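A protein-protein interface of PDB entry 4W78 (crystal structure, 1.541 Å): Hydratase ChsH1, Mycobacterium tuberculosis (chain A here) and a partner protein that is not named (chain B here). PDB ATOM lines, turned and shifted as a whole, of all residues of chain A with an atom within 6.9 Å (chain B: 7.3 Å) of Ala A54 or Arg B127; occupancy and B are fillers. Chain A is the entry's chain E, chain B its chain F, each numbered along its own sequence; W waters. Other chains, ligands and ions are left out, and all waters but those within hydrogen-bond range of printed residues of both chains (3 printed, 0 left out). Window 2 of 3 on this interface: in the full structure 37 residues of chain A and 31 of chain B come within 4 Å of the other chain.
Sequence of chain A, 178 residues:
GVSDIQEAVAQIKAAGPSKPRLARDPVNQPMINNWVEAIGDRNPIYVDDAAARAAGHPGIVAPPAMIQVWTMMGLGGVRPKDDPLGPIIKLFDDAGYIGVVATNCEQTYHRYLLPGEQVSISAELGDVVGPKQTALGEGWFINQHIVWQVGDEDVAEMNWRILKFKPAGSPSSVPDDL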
ATOM      1  N   ILE A  45      29.124  -6.138 -17.685  1.00  0.00           N
ATOM      2  CA  ILE A  45      30.081  -5.249 -17.042  1.00  0.00           C
ATOM      3  C   ILE A  45      30.694  -5.843 -15.763  1.00  0.00           C
ATOM      4  O   ILE A  45      31.710  -5.341 -15.276  1.00  0.00           O
ATOM      5  CB  ILE A  45      29.489  -3.863 -16.761  1.00  0.00           C
ATOM      6  CG1 ILE A  45      28.533  -3.921 -15.561  1.00  0.00           C
ATOM      7  CG2 ILE A  45      28.824  -3.282 -18.034  1.00  0.00           C
ATOM      8  CD1 ILE A  45      27.891  -2.563 -15.249  1.00  0.00           C
ATOM      9  N   ASP A  49      35.957  -6.867 -19.044  1.00  0.00           N
ATOM     10  CA  ASP A  49      36.519  -5.523 -18.951  1.00  0.00           C
ATOM     11  C   ASP A  49      36.069  -4.646 -20.109  1.00  0.00           C
ATOM     12  O   ASP A  49      35.785  -3.468 -19.906  1.00  0.00           O
ATOM     13  CB  ASP A  49      38.047  -5.545 -18.956  1.00  0.00           C
ATOM     14  CG  ASP A  49      38.648  -5.873 -17.601  1.00  0.00           C
ATOM     15  OD1 ASP A  49      38.060  -5.540 -16.544  1.00  0.00           O
ATOM     16  OD2 ASP A  49      39.743  -6.472 -17.600  1.00  0.00           O
ATOM     17  N   ALA A  50      36.015  -5.210 -21.318  1.00  0.00           N
ATOM     18  CA  ALA A  50      35.689  -4.404 -22.494  1.00  0.00           C
ATOM     19  C   ALA A  50      34.247  -3.920 -22.455  1.00  0.00           C
ATOM     20  O   ALA A  50      33.936  -2.793 -22.859  1.00  0.00           O
ATOM     21  CB  ALA A  50      35.973  -5.179 -23.798  1.00  0.00           C
ATOM     22  N   ALA A  51      33.361  -4.771 -21.953  1.00  0.00           N
ATOM     23  CA  ALA A  51      31.971  -4.378 -21.821  1.00  0.00           C
ATOM     24  C   ALA A  51      31.859  -3.281 -20.796  1.00  0.00           C
ATOM     25  O   ALA A  51      31.108  -2.332 -20.981  1.00  0.00           O
ATOM     26  CB  ALA A  51      31.106  -5.561 -21.420  1.00  0.00           C
ATOM     27  N   ALA A  52      32.573  -3.438 -19.682  1.00  0.00           N
ATOM     28  CA  ALA A  52      32.542  -2.421 -18.641  1.00  0.00           C
ATOM     29  C   ALA A  52      33.050  -1.079 -19.166  1.00  0.00           C
ATOM     30  O   ALA A  52      32.512  -0.031 -18.840  1.00  0.00           O
ATOM     31  CB  ALA A  52      33.345  -2.872 -17.436  1.00  0.00           C
ATOM     32  N   ARG A  53      34.070  -1.121 -20.012  1.00  0.00           N
ATOM     33  CA  ARG A  53      34.568   0.128 -20.595  1.00  0.00           C
ATOM     34  C   ARG A  53      33.597   0.766 -21.588  1.00  0.00           C
ATOM     35  O   ARG A  53      33.514   1.993 -21.677  1.00  0.00           O
ATOM     36  CB  ARG A  53      35.949  -0.069 -21.227  1.00  0.00           C
ATOM     37  CG  ARG A  53      37.011  -0.376 -20.190  1.00  0.00           C
ATOM     38  CD  ARG A  53      38.418  -0.515 -20.752  1.00  0.00           C
ATOM     39  NE  ARG A  53      39.302  -0.916 -19.662  1.00  0.00           N
ATOM     40  CZ  ARG A  53      39.922  -2.090 -19.574  1.00  0.00           C
ATOM     41  NH1 ARG A  53      39.814  -2.986 -20.545  1.00  0.00           N
ATOM     42  NH2 ARG A  53      40.681  -2.348 -18.520  1.00  0.00           N
ATOM     43  N   ALA A  54      32.863  -0.053 -22.338  1.00  0.00           N
ATOM     44  CA  ALA A  54      31.866   0.496 -23.268  1.00  0.00           C
ATOM     45  C   ALA A  54      30.739   1.173 -22.493  1.00  0.00           C
ATOM     46  O   ALA A  54      30.013   2.018 -23.023  1.00  0.00           O
ATOM     47  CB  ALA A  54      31.320  -0.588 -24.162  1.00  0.00           C
ATOM     48  N   ALA A  55      30.612   0.805 -21.227  1.00  0.00           N
ATOM     49  CA  ALA A  55      29.604   1.398 -20.367  1.00  0.00           C
ATOM     50  C   ALA A  55      30.181   2.539 -19.535  1.00  0.00           C
ATOM     51  O   ALA A  55      29.515   3.045 -18.644  1.00  0.00           O
ATOM     52  CB  ALA A  55      28.970   0.332 -19.466  1.00  0.00           C
ATOM     53  N   GLY A  56      31.426   2.927 -19.809  1.00  0.00           N
ATOM     54  CA  GLY A  56      32.009   4.098 -19.165  1.00  0.00           C
ATOM     55  C   GLY A  56      32.811   3.864 -17.892  1.00  0.00           C
ATOM     56  O   GLY A  56      33.265   4.824 -17.258  1.00  0.00           O
ATOM     57  N   HIS A  57      33.020   2.598 -17.536  1.00  0.00           N
ATOM     58  CA  HIS A  57      33.794   2.244 -16.341  1.00  0.00           C
ATOM     59  C   HIS A  57      35.247   1.970 -16.699  1.00  0.00           C
ATOM     60  O   HIS A  57      35.558   1.698 -17.848  1.00  0.00           O
ATOM     61  CB  HIS A  57      33.211   0.993 -15.684  1.00  0.00           C
ATOM     62  CG  HIS A  57      31.777   1.132 -15.297  1.00  0.00           C
ATOM     63  ND1 HIS A  57      31.372   1.853 -14.193  1.00  0.00           N
ATOM     64  CD2 HIS A  57      30.651   0.634 -15.858  1.00  0.00           C
ATOM     65  CE1 HIS A  57      30.057   1.785 -14.086  1.00  0.00           C
ATOM     66  NE2 HIS A  57      29.593   1.056 -15.086  1.00  0.00           N
ATOM     67  N   ALA B  67      17.365  -2.162 -18.905  1.00  0.00           N
ATOM     68  CA  ALA B  67      18.039  -0.877 -19.091  1.00  0.00           C
ATOM     69  C   ALA B  67      19.354  -1.014 -19.844  1.00  0.00           C
ATOM     70  O   ALA B  67      19.780  -0.093 -20.552  1.00  0.00           O
ATOM     71  CB  ALA B  67      18.258  -0.200 -17.728  1.00  0.00           C
ATOM     72  N   PRO B  69      23.633  -2.531 -20.114  1.00  0.00           N
ATOM     73  CA  PRO B  69      24.928  -2.450 -19.434  1.00  0.00           C
ATOM     74  C   PRO B  69      25.343  -1.037 -19.044  1.00  0.00           C
ATOM     75  O   PRO B  69      26.120  -0.911 -18.101  1.00  0.00           O
ATOM     76  CB  PRO B  69      25.920  -3.002 -20.469  1.00  0.00           C
ATOM     77  CG  PRO B  69      25.107  -3.576 -21.569  1.00  0.00           C
ATOM     78  CD  PRO B  69      23.761  -2.960 -21.517  1.00  0.00           C
ATOM     79  N   SER B  70      24.850  -0.012 -19.739  1.00  0.00           N
ATOM     80  CA  SER B  70      25.252   1.359 -19.433  1.00  0.00           C
ATOM     81  C   SER B  70      24.477   1.944 -18.256  1.00  0.00           C
ATOM     82  O   SER B  70      24.785   3.042 -17.786  1.00  0.00           O
ATOM     83  CB  SER B  70      25.083   2.260 -20.661  1.00  0.00           C
ATOM     84  OG  SER B  70      23.716   2.350 -21.013  1.00  0.00           O
ATOM     85  N   ALA B  71      23.465   1.219 -17.788  1.00  0.00           N
ATOM     86  CA  ALA B  71      22.641   1.707 -16.689  1.00  0.00           C
ATOM     87  C   ALA B  71      23.484   1.820 -15.437  1.00  0.00           C
ATOM     88  O   ALA B  71      24.309   0.945 -15.160  1.00  0.00           O
ATOM     89  CB  ALA B  71      21.483   0.777 -16.451  1.00  0.00           C
ATOM     90  N   LEU B  72      23.263   2.888 -14.672  1.00  0.00           N
ATOM     91  CA  LEU B  72      23.949   3.070 -13.399  1.00  0.00           C
ATOM     92  C   LEU B  72      22.920   3.077 -12.280  1.00  0.00           C
ATOM     93  O   LEU B  72      22.139   4.026 -12.155  1.00  0.00           O
ATOM     94  CB  LEU B  72      24.730   4.385 -13.395  1.00  0.00           C
ATOM     95  CG  LEU B  72      25.886   4.491 -14.371  1.00  0.00           C
ATOM     96  CD1 LEU B  72      26.379   5.936 -14.420  1.00  0.00           C
ATOM     97  CD2 LEU B  72      27.003   3.545 -13.953  1.00  0.00           C
ATOM     98  N   GLY B 102      17.734  12.435 -17.016  1.00  0.00           N
ATOM     99  CA  GLY B 102      18.651  11.307 -17.005  1.00  0.00           C
ATOM    100  C   GLY B 102      18.381  10.298 -15.888  1.00  0.00           C
ATOM    101  O   GLY B 102      18.744   9.115 -15.997  1.00  0.00           O
ATOM    102  N   ILE B 104      16.001   8.032 -13.671  1.00  0.00           N
ATOM    103  CA  ILE B 104      14.762   7.298 -13.891  1.00  0.00           C
ATOM    104  C   ILE B 104      14.397   6.565 -12.618  1.00  0.00           C
ATOM    105  O   ILE B 104      15.274   6.077 -11.917  1.00  0.00           O
ATOM    106  CB  ILE B 104      14.958   6.272 -15.021  1.00  0.00           C
ATOM    107  CG1 ILE B 104      15.238   7.003 -16.331  1.00  0.00           C
ATOM    108  CG2 ILE B 104      13.747   5.358 -15.176  1.00  0.00           C
ATOM    109  CD1 ILE B 104      16.207   6.305 -17.223  1.00  0.00           C
ATOM    110  N   SER B 125      20.405   5.905 -13.556  1.00  0.00           N
ATOM    111  CA  SER B 125      20.606   6.767 -14.709  1.00  0.00           C
ATOM    112  C   SER B 125      20.835   5.850 -15.897  1.00  0.00           C
ATOM    113  O   SER B 125      21.434   4.782 -15.765  1.00  0.00           O
ATOM    114  CB  SER B 125      21.811   7.668 -14.494  1.00  0.00           C
ATOM    115  OG  SER B 125      22.998   6.907 -14.558  1.00  0.00           O
ATOM    116  N   MET B 126      20.339   6.252 -17.058  1.00  0.00           N
ATOM    117  CA  MET B 126      20.492   5.433 -18.240  1.00  0.00           C
ATOM    118  C   MET B 126      21.070   6.303 -19.338  1.00  0.00           C
ATOM    119  O   MET B 126      20.839   7.510 -19.369  1.00  0.00           O
ATOM    120  CB  MET B 126      19.148   4.843 -18.672  1.00  0.00           C
ATOM    121  CG  MET B 126      19.267   3.541 -19.455  1.00  0.00           C
ATOM    122  SD  MET B 126      17.673   2.913 -20.024  1.00  0.00           S
ATOM    123  CE  MET B 126      16.678   3.165 -18.575  1.00  0.00           C
ATOM    124  N   ARG B 127      21.831   5.687 -20.230  1.00  0.00           N
ATOM    125  CA  ARG B 127      22.509   6.414 -21.289  1.00  0.00           C
ATOM    126  C   ARG B 127      21.818   6.142 -22.613  1.00  0.00           C
ATOM    127  O   ARG B 127      21.106   5.149 -22.750  1.00  0.00           O
ATOM    128  CB  ARG B 127      23.964   5.963 -21.355  1.00  0.00           C
ATOM    129  CG  ARG B 127      24.905   6.908 -22.048  1.00  0.00           C
ATOM    130  CD  ARG B 127      26.270   6.253 -22.141  1.00  0.00           C
ATOM    131  NE  ARG B 127      26.209   5.004 -22.897  1.00  0.00           N
ATOM    132  CZ  ARG B 127      27.164   4.079 -22.894  1.00  0.00           C
ATOM    133  NH1 ARG B 127      28.252   4.251 -22.160  1.00  0.00           N
ATOM    134  NH2 ARG B 127      27.023   2.976 -23.613  1.00  0.00           N
HETATM  135  O   HOH W   1      29.687   2.875 -25.613  1.00  0.00           O
HETATM  136  O   HOH W   2      27.495   3.912 -17.433  1.00  0.00           O
HETATM  137  O   HOH W   3      26.984   0.834 -16.185  1.00  0.00           O
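The backbone carbonyl oxygen (O) of Ala A54 is in hydrogen-bond range of the guanidinium group (NH1) of Arg B127, 3.0 Å away.
The backbone carbonyl oxygen (O) of Ser B125 sits at hydrogen-bond distance from the backbone NH (N) of Leu B72. The backbone carbonyl oxygen (O) of Ala A52 lies within hydrogen-bond range of the backbone NH (N) of His A57.
CG2 of Ile A45 touches O of Pro B69, 3.6 Å away. Ala A55 touches Pro B69. CB of Ala A55 touches CA of Ser B70, 3.9 Å away. NH1 of Arg B127 touches CA of Ala A55 (3.6 Å). Leu B72 touches His A57 (CD2 to CE1, 3.5 Å).
Ala A54 touches one residue of chain B. Arg B127 touches two residues of chain A. Printed residues of chain B within 4 Å of Ala A55: Pro B69, Ser B70 and Arg B127. Of the printed residues of chain B, Ile A45 touches Pro B69. Ser B125 touches none of the printed residues of chain A. The nearest residue of chain A that does not touch Arg B127 is Gly A56 (4.2 Å). The nearest printed residue of chain B that does not touch Ala A55 is Leu B72 (5.3 Å).
Of the 10 printed residues of chain A, 4 touch a printed residue of chain B. Hydrophobic or aromatic side chains of chain B that line the printed part of chain A: Pro B69 and Leu B72.
Water W2 lies within hydrogen-bond range of O of Ala A55 (2.5 Å) and O of Ser B70 (2.9 Å). Water W3 lies within hydrogen-bond range of the backbone carbonyl oxygen (O) of Pro B69 (2.7 Å), a ring nitrogen (NE2) of His A57 (2.8 Å) and the backbone carbonyl oxygen (O) of Ala B71 (2.9 Å). Water W1 lies within hydrogen-bond range of O of Ala A54 (2.7 Å) and NH2 of Arg B127 (3.3 Å).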
